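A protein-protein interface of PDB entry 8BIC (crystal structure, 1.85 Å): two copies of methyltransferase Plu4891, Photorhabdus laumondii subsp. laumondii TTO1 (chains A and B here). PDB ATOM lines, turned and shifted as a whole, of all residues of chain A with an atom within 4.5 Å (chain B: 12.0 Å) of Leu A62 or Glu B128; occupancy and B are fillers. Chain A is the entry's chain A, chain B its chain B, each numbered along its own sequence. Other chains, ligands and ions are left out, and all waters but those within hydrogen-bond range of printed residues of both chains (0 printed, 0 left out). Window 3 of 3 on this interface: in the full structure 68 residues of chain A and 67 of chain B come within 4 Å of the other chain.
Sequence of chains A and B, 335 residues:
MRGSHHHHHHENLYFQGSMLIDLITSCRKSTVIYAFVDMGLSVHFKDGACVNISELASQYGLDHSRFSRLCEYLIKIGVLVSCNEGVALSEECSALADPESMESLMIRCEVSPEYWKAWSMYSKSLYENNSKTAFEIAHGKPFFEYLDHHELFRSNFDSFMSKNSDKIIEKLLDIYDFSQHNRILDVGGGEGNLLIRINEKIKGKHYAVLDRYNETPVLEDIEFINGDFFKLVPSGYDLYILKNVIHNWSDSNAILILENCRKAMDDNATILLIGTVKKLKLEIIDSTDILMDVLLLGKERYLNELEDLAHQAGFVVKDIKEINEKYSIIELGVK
Of the 9 printed residues of chain A, 5 touch a printed residue of chain B.
Printed residues of chain A that touch a printed residue of chain B: Met A39, Tyr A60, Gly A61, Leu A62 and Asp A63.
Hydrophobic or aromatic side chains of chain B that line the printed part of chain A: Leu B126 and Tyr B127.
Among the printed residues, no Asp or Glu carboxylate lies within 4 Å of a Lys or Arg side-chain nitrogen of the other chain.
Leu A62 touches just these residues of chain B: Leu B126, Tyr B127 and Glu B128.
Of the printed residues of chain A, Glu B128 touches Gly A61 (2.6 Å), Leu A62 (3.0 Å) and Asp A63 (3.8 Å).
Of chain B, only Tyr B127 (3.4 Å) comes within 4 Å of Tyr A60.
Asp A63 touches two residues of chain B.
Printed residues of chain A within 4 Å of Ser B123: Met A39 (3.8 Å).
Of the printed residues of chain A, Leu B126 touches Met A39, Leu A62 and Asp A63.
Printed residues of chain A within 4 Å of Tyr B127: Met A39 (3.4 Å), Tyr A60 (3.4 Å), Gly A61 (3.3 Å) and Leu A62 (3.7 Å).
Asp B293 touches none of the printed residues of chain A.
The nearest residue of chain A that does not touch Glu B128 is Ala A57 (4.3 Å).
The nearest printed residue of chain A that does not touch Ser B123 is Leu A62 (5.3 Å).
N of Leu A62 is in hydrogen-bond range of O of Ala A57 (2.7 Å).
The backbone carbonyl oxygen of Tyr B127 lies close to the side-chain amide oxygen of Asn B129, at 3.4 Å.
O of Tyr B127 sits close to OD1 of Asn B130 (2.9 Å).
The backbone carbonyl oxygen (O) of Met A39 is in hydrogen-bond range of the side-chain hydroxyl (OH) of Tyr B127 (3.4 Å).
The backbone carbonyl oxygen of Gly A61 lies within hydrogen-bond range of the backbone NH of Glu B128, 2.6 Å away.
N of Asp A63 sits at hydrogen-bond distance from O of Leu B126 (2.8 Å).
The backbone carbonyl oxygen of Leu A62 sits close to the side-chain carboxylate of Glu B128, at 3.0 Å.
No position is printed for both chains.
Of the 11 pairs that touch across the chains among the printed residues, none has its exchanged pair printed and touching as well.
CG of Met A39 touches CB of Ser B123, at 3.8 Å.
Met A39 touches Leu B126.
Tyr B127 touches Tyr A60.
CA of Tyr B127 touches O of Gly A61, 3.3 Å away.
CA of Leu A62 touches O of Leu B126, at 3.3 Å.
Leu A62 touches Tyr B127.
N of Asp A63 touches N of Glu B128, at 3.8 Å.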
ATOM      1  N   MET A  39      31.628 -16.952 -10.697  1.00  0.00           N
ATOM      2  CA  MET A  39      31.602 -16.804  -9.215  1.00  0.00           C
ATOM      3  C   MET A  39      32.796 -15.977  -8.719  1.00  0.00           C
ATOM      4  O   MET A  39      32.753 -15.550  -7.554  1.00  0.00           O
ATOM      5  CB  MET A  39      31.592 -18.177  -8.541  1.00  0.00           C
ATOM      6  CG  MET A  39      30.254 -18.863  -8.680  1.00  0.00           C
ATOM      7  SD  MET A  39      30.194 -20.494  -7.928  1.00  0.00           S
ATOM      8  CE  MET A  39      29.703 -20.055  -6.264  1.00  0.00           C
ATOM      9  N   LEU A  56      36.228 -21.601   1.586  1.00  0.00           N
ATOM     10  CA  LEU A  56      35.828 -20.852   0.364  1.00  0.00           C
ATOM     11  C   LEU A  56      34.353 -20.444   0.459  1.00  0.00           C
ATOM     12  O   LEU A  56      34.048 -19.275   0.147  1.00  0.00           O
ATOM     13  CB  LEU A  56      36.084 -21.732  -0.863  1.00  0.00           C
ATOM     14  CG  LEU A  56      36.192 -20.994  -2.197  1.00  0.00           C
ATOM     15  CD1 LEU A  56      37.401 -20.070  -2.222  1.00  0.00           C
ATOM     16  CD2 LEU A  56      36.263 -21.985  -3.345  1.00  0.00           C
ATOM     17  N   ALA A  57      33.478 -21.368   0.873  1.00  0.00           N
ATOM     18  CA  ALA A  57      32.014 -21.163   0.966  1.00  0.00           C
ATOM     19  C   ALA A  57      31.695 -20.141   2.064  1.00  0.00           C
ATOM     20  O   ALA A  57      30.836 -19.272   1.823  1.00  0.00           O
ATOM     21  CB  ALA A  57      31.317 -22.476   1.222  1.00  0.00           C
ATOM     22  N   TYR A  60      32.927 -16.407   0.939  1.00  0.00           N
ATOM     23  CA  TYR A  60      32.111 -15.869  -0.184  1.00  0.00           C
ATOM     24  C   TYR A  60      30.623 -15.816   0.183  1.00  0.00           C
ATOM     25  O   TYR A  60      29.856 -15.145  -0.542  1.00  0.00           O
ATOM     26  CB  TYR A  60      32.303 -16.733  -1.432  1.00  0.00           C
ATOM     27  CG  TYR A  60      33.393 -16.264  -2.359  1.00  0.00           C
ATOM     28  CD1 TYR A  60      34.559 -15.695  -1.868  1.00  0.00           C
ATOM     29  CD2 TYR A  60      33.257 -16.391  -3.733  1.00  0.00           C
ATOM     30  CE1 TYR A  60      35.557 -15.254  -2.720  1.00  0.00           C
ATOM     31  CE2 TYR A  60      34.247 -15.958  -4.598  1.00  0.00           C
ATOM     32  CZ  TYR A  60      35.402 -15.391  -4.089  1.00  0.00           C
ATOM     33  OH  TYR A  60      36.382 -14.963  -4.933  1.00  0.00           O
ATOM     34  N   GLY A  61      30.225 -16.506   1.254  1.00  0.00           N
ATOM     35  CA  GLY A  61      28.807 -16.753   1.572  1.00  0.00           C
ATOM     36  C   GLY A  61      28.167 -17.608   0.493  1.00  0.00           C
ATOM     37  O   GLY A  61      27.215 -17.128  -0.150  1.00  0.00           O
ATOM     38  N   LEU A  62      28.696 -18.821   0.287  1.00  0.00           N
ATOM     39  CA  LEU A  62      28.155 -19.852  -0.643  1.00  0.00           C
ATOM     40  C   LEU A  62      27.531 -20.994   0.167  1.00  0.00           C
ATOM     41  O   LEU A  62      28.020 -21.265   1.279  1.00  0.00           O
ATOM     42  CB  LEU A  62      29.283 -20.399  -1.524  1.00  0.00           C
ATOM     43  CG  LEU A  62      29.990 -19.386  -2.418  1.00  0.00           C
ATOM     44  CD1 LEU A  62      31.151 -20.041  -3.148  1.00  0.00           C
ATOM     45  CD2 LEU A  62      29.019 -18.765  -3.410  1.00  0.00           C
ATOM     46  N   ASP A  63      26.512 -21.654  -0.389  1.00  0.00           N
ATOM     47  CA  ASP A  63      25.932 -22.902   0.174  1.00  0.00           C
ATOM     48  C   ASP A  63      26.983 -24.014   0.055  1.00  0.00           C
ATOM     49  O   ASP A  63      27.349 -24.368  -1.082  1.00  0.00           O
ATOM     50  CB  ASP A  63      24.625 -23.269  -0.528  1.00  0.00           C
ATOM     51  CG  ASP A  63      23.888 -24.421   0.132  1.00  0.00           C
ATOM     52  OD1 ASP A  63      22.801 -24.173   0.683  1.00  0.00           O
ATOM     53  OD2 ASP A  63      24.407 -25.556   0.086  1.00  0.00           O
ATOM     54  N   HIS A  64      27.456 -24.536   1.188  1.00  0.00           N
ATOM     55  CA  HIS A  64      28.584 -25.503   1.267  1.00  0.00           C
ATOM     56  C   HIS A  64      28.257 -26.775   0.471  1.00  0.00           C
ATOM     57  O   HIS A  64      29.043 -27.119  -0.437  1.00  0.00           O
ATOM     58  CB  HIS A  64      28.932 -25.816   2.728  1.00  0.00           C
ATOM     59  CG  HIS A  64      29.845 -26.984   2.880  1.00  0.00           C
ATOM     60  ND1 HIS A  64      31.133 -26.985   2.376  1.00  0.00           N
ATOM     61  CD2 HIS A  64      29.663 -28.189   3.463  1.00  0.00           C
ATOM     62  CE1 HIS A  64      31.709 -28.138   2.650  1.00  0.00           C
ATOM     63  NE2 HIS A  64      30.828 -28.895   3.319  1.00  0.00           N
ATOM     64  N   PHE A  67      27.758 -26.279  -3.300  1.00  0.00           N
ATOM     65  CA  PHE A  67      29.063 -25.936  -3.927  1.00  0.00           C
ATOM     66  C   PHE A  67      29.948 -27.187  -3.987  1.00  0.00           C
ATOM     67  O   PHE A  67      30.660 -27.359  -4.990  1.00  0.00           O
ATOM     68  CB  PHE A  67      29.762 -24.790  -3.193  1.00  0.00           C
ATOM     69  CG  PHE A  67      31.089 -24.406  -3.797  1.00  0.00           C
ATOM     70  CD1 PHE A  67      31.156 -23.767  -5.025  1.00  0.00           C
ATOM     71  CD2 PHE A  67      32.275 -24.703  -3.145  1.00  0.00           C
ATOM     72  CE1 PHE A  67      32.378 -23.427  -5.583  1.00  0.00           C
ATOM     73  CE2 PHE A  67      33.498 -24.363  -3.705  1.00  0.00           C
ATOM     74  CZ  PHE A  67      33.547 -23.725  -4.923  1.00  0.00           C
ATOM     75  N   MET B 121      22.281 -18.279 -14.375  1.00  0.00           N
ATOM     76  CA  MET B 121      21.990 -17.775 -13.002  1.00  0.00           C
ATOM     77  C   MET B 121      22.397 -18.787 -11.923  1.00  0.00           C
ATOM     78  O   MET B 121      22.141 -18.514 -10.734  1.00  0.00           O
ATOM     79  CB  MET B 121      20.498 -17.461 -12.877  1.00  0.00           C
ATOM     80  CG  MET B 121      20.066 -16.316 -13.778  1.00  0.00           C
ATOM     81  SD  MET B 121      20.898 -14.778 -13.320  1.00  0.00           S
ATOM     82  CE  MET B 121      22.170 -14.643 -14.570  1.00  0.00           C
ATOM     83  N   TYR B 122      23.031 -19.898 -12.307  1.00  0.00           N
ATOM     84  CA  TYR B 122      23.499 -20.963 -11.382  1.00  0.00           C
ATOM     85  C   TYR B 122      24.510 -20.378 -10.385  1.00  0.00           C
ATOM     86  O   TYR B 122      24.391 -20.658  -9.177  1.00  0.00           O
ATOM     87  CB  TYR B 122      24.079 -22.128 -12.183  1.00  0.00           C
ATOM     88  CG  TYR B 122      24.658 -23.252 -11.362  1.00  0.00           C
ATOM     89  CD1 TYR B 122      24.083 -23.659 -10.167  1.00  0.00           C
ATOM     90  CD2 TYR B 122      25.773 -23.942 -11.811  1.00  0.00           C
ATOM     91  CE1 TYR B 122      24.614 -24.707  -9.430  1.00  0.00           C
ATOM     92  CE2 TYR B 122      26.313 -24.991 -11.088  1.00  0.00           C
ATOM     93  CZ  TYR B 122      25.734 -25.374  -9.893  1.00  0.00           C
ATOM     94  OH  TYR B 122      26.273 -26.407  -9.184  1.00  0.00           O
ATOM     95  N   SER B 123      25.463 -19.585 -10.880  1.00  0.00           N
ATOM     96  CA  SER B 123      26.489 -18.869 -10.078  1.00  0.00           C
ATOM     97  C   SER B 123      25.821 -18.004  -9.001  1.00  0.00           C
ATOM     98  O   SER B 123      26.320 -18.007  -7.853  1.00  0.00           O
ATOM     99  CB  SER B 123      27.375 -18.041 -10.969  1.00  0.00           C
ATOM    100  OG  SER B 123      26.604 -17.137 -11.754  1.00  0.00           O
ATOM    101  N   LYS B 124      24.736 -17.299  -9.349  1.00  0.00           N
ATOM    102  CA  LYS B 124      24.017 -16.367  -8.431  1.00  0.00           C
ATOM    103  C   LYS B 124      23.181 -17.164  -7.424  1.00  0.00           C
ATOM    104  O   LYS B 124      22.973 -16.654  -6.304  1.00  0.00           O
ATOM    105  CB  LYS B 124      23.113 -15.400  -9.206  1.00  0.00           C
ATOM    106  CG  LYS B 124      23.780 -14.630 -10.339  1.00  0.00           C
ATOM    107  CD  LYS B 124      25.086 -13.958  -9.957  1.00  0.00           C
ATOM    108  CE  LYS B 124      25.903 -13.525 -11.155  1.00  0.00           C
ATOM    109  NZ  LYS B 124      27.268 -13.107 -10.756  1.00  0.00           N
ATOM    110  N   SER B 125      22.713 -18.357  -7.798  1.00  0.00           N
ATOM    111  CA  SER B 125      21.847 -19.220  -6.947  1.00  0.00           C
ATOM    112  C   SER B 125      22.655 -19.855  -5.803  1.00  0.00           C
ATOM    113  O   SER B 125      22.041 -20.222  -4.788  1.00  0.00           O
ATOM    114  CB  SER B 125      21.145 -20.273  -7.766  1.00  0.00           C
ATOM    115  OG  SER B 125      22.028 -21.341  -8.076  1.00  0.00           O
ATOM    116  N   LEU B 126      23.976 -19.989  -5.957  1.00  0.00           N
ATOM    117  CA  LEU B 126      24.841 -20.748  -5.013  1.00  0.00           C
ATOM    118  C   LEU B 126      25.160 -19.903  -3.773  1.00  0.00           C
ATOM    119  O   LEU B 126      25.657 -20.481  -2.784  1.00  0.00           O
ATOM    120  CB  LEU B 126      26.117 -21.199  -5.732  1.00  0.00           C
ATOM    121  CG  LEU B 126      25.948 -22.426  -6.628  1.00  0.00           C
ATOM    122  CD1 LEU B 126      27.174 -22.637  -7.502  1.00  0.00           C
ATOM    123  CD2 LEU B 126      25.663 -23.674  -5.802  1.00  0.00           C
ATOM    124  N   TYR B 127      24.874 -18.599  -3.809  1.00  0.00           N
ATOM    125  CA  TYR B 127      25.159 -17.663  -2.691  1.00  0.00           C
ATOM    126  C   TYR B 127      24.219 -17.989  -1.525  1.00  0.00           C
ATOM    127  O   TYR B 127      22.987 -18.012  -1.719  1.00  0.00           O
ATOM    128  CB  TYR B 127      25.140 -16.211  -3.179  1.00  0.00           C
ATOM    129  CG  TYR B 127      26.423 -15.817  -3.871  1.00  0.00           C
ATOM    130  CD1 TYR B 127      27.511 -15.346  -3.151  1.00  0.00           C
ATOM    131  CD2 TYR B 127      26.576 -15.974  -5.240  1.00  0.00           C
ATOM    132  CE1 TYR B 127      28.701 -15.007  -3.773  1.00  0.00           C
ATOM    133  CE2 TYR B 127      27.761 -15.642  -5.880  1.00  0.00           C
ATOM    134  CZ  TYR B 127      28.830 -15.157  -5.145  1.00  0.00           C
ATOM    135  OH  TYR B 127      29.996 -14.833  -5.781  1.00  0.00           O
ATOM    136  N   GLU B 128      24.836 -18.264  -0.367  1.00  0.00           N
ATOM    137  CA  GLU B 128      24.247 -18.763   0.911  1.00  0.00           C
ATOM    138  C   GLU B 128      22.988 -17.967   1.277  1.00  0.00           C
ATOM    139  O   GLU B 128      22.005 -18.592   1.731  1.00  0.00           O
ATOM    140  CB  GLU B 128      25.292 -18.629   2.023  1.00  0.00           C
ATOM    141  CG  GLU B 128      25.179 -19.649   3.136  1.00  0.00           C
ATOM    142  CD  GLU B 128      26.294 -19.513   4.159  1.00  0.00           C
ATOM    143  OE1 GLU B 128      26.183 -18.632   5.039  1.00  0.00           O
ATOM    144  OE2 GLU B 128      27.292 -20.262   4.052  1.00  0.00           O
ATOM    145  N   ASN B 129      23.036 -16.643   1.096  1.00  0.00           N
ATOM    146  CA  ASN B 129      21.969 -15.678   1.485  1.00  0.00           C
ATOM    147  C   ASN B 129      20.694 -15.908   0.657  1.00  0.00           C
ATOM    148  O   ASN B 129      19.607 -15.544   1.152  1.00  0.00           O
ATOM    149  CB  ASN B 129      22.442 -14.225   1.355  1.00  0.00           C
ATOM    150  CG  ASN B 129      22.872 -13.849  -0.050  1.00  0.00           C
ATOM    151  OD1 ASN B 129      23.031 -14.711  -0.912  1.00  0.00           O
ATOM    152  ND2 ASN B 129      23.072 -12.563  -0.288  1.00  0.00           N
ATOM    153  N   ASN B 130      20.813 -16.469  -0.552  1.00  0.00           N
ATOM    154  CA  ASN B 130      19.674 -16.662  -1.494  1.00  0.00           C
ATOM    155  C   ASN B 130      18.988 -18.003  -1.195  1.00  0.00           C
ATOM    156  O   ASN B 130      19.666 -18.911  -0.666  1.00  0.00           O
ATOM    157  CB  ASN B 130      20.126 -16.569  -2.955  1.00  0.00           C
ATOM    158  CG  ASN B 130      20.079 -17.899  -3.676  1.00  0.00           C
ATOM    159  OD1 ASN B 130      20.687 -18.875  -3.238  1.00  0.00           O
ATOM    160  ND2 ASN B 130      19.347 -17.949  -4.774  1.00  0.00           N
ATOM    161  N   SER B 131      17.696 -18.117  -1.527  1.00  0.00           N
ATOM    162  CA  SER B 131      16.883 -19.359  -1.390  1.00  0.00           C
ATOM    163  C   SER B 131      16.067 -19.644  -2.666  1.00  0.00           C
ATOM    164  O   SER B 131      15.235 -20.577  -2.635  1.00  0.00           O
ATOM    165  CB  SER B 131      15.997 -19.275  -0.169  1.00  0.00           C
ATOM    166  OG  SER B 131      15.111 -18.172  -0.256  1.00  0.00           O
ATOM    167  N   LYS B 132      16.301 -18.908  -3.758  1.00  0.00           N
ATOM    168  CA  LYS B 132      15.571 -19.075  -5.047  1.00  0.00           C
ATOM    169  C   LYS B 132      16.348 -20.032  -5.957  1.00  0.00           C
ATOM    170  O   LYS B 132      17.594 -20.010  -5.899  1.00  0.00           O
ATOM    171  CB  LYS B 132      15.388 -17.725  -5.748  1.00  0.00           C
ATOM    172  CG  LYS B 132      14.275 -16.850  -5.192  1.00  0.00           C
ATOM    173  CD  LYS B 132      14.000 -15.621  -6.035  1.00  0.00           C
ATOM    174  CE  LYS B 132      14.850 -14.428  -5.651  1.00  0.00           C
ATOM    175  NZ  LYS B 132      14.763 -13.354  -6.670  1.00  0.00           N
ATOM    176  N   THR B 133      15.651 -20.823  -6.780  1.00  0.00           N
ATOM    177  CA  THR B 133      16.282 -21.675  -7.829  1.00  0.00           C
ATOM    178  C   THR B 133      16.903 -20.758  -8.883  1.00  0.00           C
ATOM    179  O   THR B 133      16.399 -19.629  -9.058  1.00  0.00           O
ATOM    180  CB  THR B 133      15.308 -22.665  -8.484  1.00  0.00           C
ATOM    181  OG1 THR B 133      14.328 -21.934  -9.221  1.00  0.00           O
ATOM    182  CG2 THR B 133      14.643 -23.588  -7.484  1.00  0.00           C
ATOM    183  N   ALA B 134      17.965 -21.217  -9.553  1.00  0.00           N
ATOM    184  CA  ALA B 134      18.598 -20.491 -10.672  1.00  0.00           C
ATOM    185  C   ALA B 134      17.520 -20.214 -11.730  1.00  0.00           C
ATOM    186  O   ALA B 134      17.536 -19.123 -12.338  1.00  0.00           O
ATOM    187  CB  ALA B 134      19.749 -21.295 -11.227  1.00  0.00           C
ATOM    188  N   ILE B 137      15.320 -17.304 -10.533  1.00  0.00           N
ATOM    189  CA  ILE B 137      16.146 -16.066 -10.667  1.00  0.00           C
ATOM    190  C   ILE B 137      16.098 -15.629 -12.135  1.00  0.00           C
ATOM    191  O   ILE B 137      15.951 -14.426 -12.394  1.00  0.00           O
ATOM    192  CB  ILE B 137      17.584 -16.286 -10.160  1.00  0.00           C
ATOM    193  CG1 ILE B 137      17.610 -16.570  -8.654  1.00  0.00           C
ATOM    194  CG2 ILE B 137      18.469 -15.096 -10.512  1.00  0.00           C
ATOM    195  CD1 ILE B 137      18.938 -17.054  -8.133  1.00  0.00           C
ATOM    196  N   ASP B 293      19.671 -29.230  -9.384  1.00  0.00           N
ATOM    197  CA  ASP B 293      19.984 -28.065  -8.515  1.00  0.00           C
ATOM    198  C   ASP B 293      19.577 -26.773  -9.238  1.00  0.00           C
ATOM    199  O   ASP B 293      18.876 -25.943  -8.631  1.00  0.00           O
ATOM    200  CB  ASP B 293      21.460 -28.025  -8.116  1.00  0.00           C
ATOM    201  CG  ASP B 293      21.705 -27.075  -6.962  1.00  0.00           C
ATOM    202  OD1 ASP B 293      20.990 -27.190  -5.972  1.00  0.00           O
ATOM    203  OD2 ASP B 293      22.573 -26.207  -7.081  1.00  0.00           O
ATOM    204  N   LEU B 297      16.355 -26.858  -7.295  1.00  0.00           N
ATOM    205  CA  LEU B 297      17.080 -27.087  -6.012  1.00  0.00           C
ATOM    206  C   LEU B 297      16.804 -28.528  -5.553  1.00  0.00           C
ATOM    207  O   LEU B 297      16.733 -28.777  -4.335  1.00  0.00           O
ATOM    208  CB  LEU B 297      16.647 -26.043  -4.969  1.00  0.00           C
ATOM    209  CG  LEU B 297      17.410 -24.717  -5.021  1.00  0.00           C
ATOM    210  CD1 LEU B 297      16.621 -23.595  -4.368  1.00  0.00           C
ATOM    211  CD2 LEU B 297      18.775 -24.845  -4.365  1.00  0.00           C
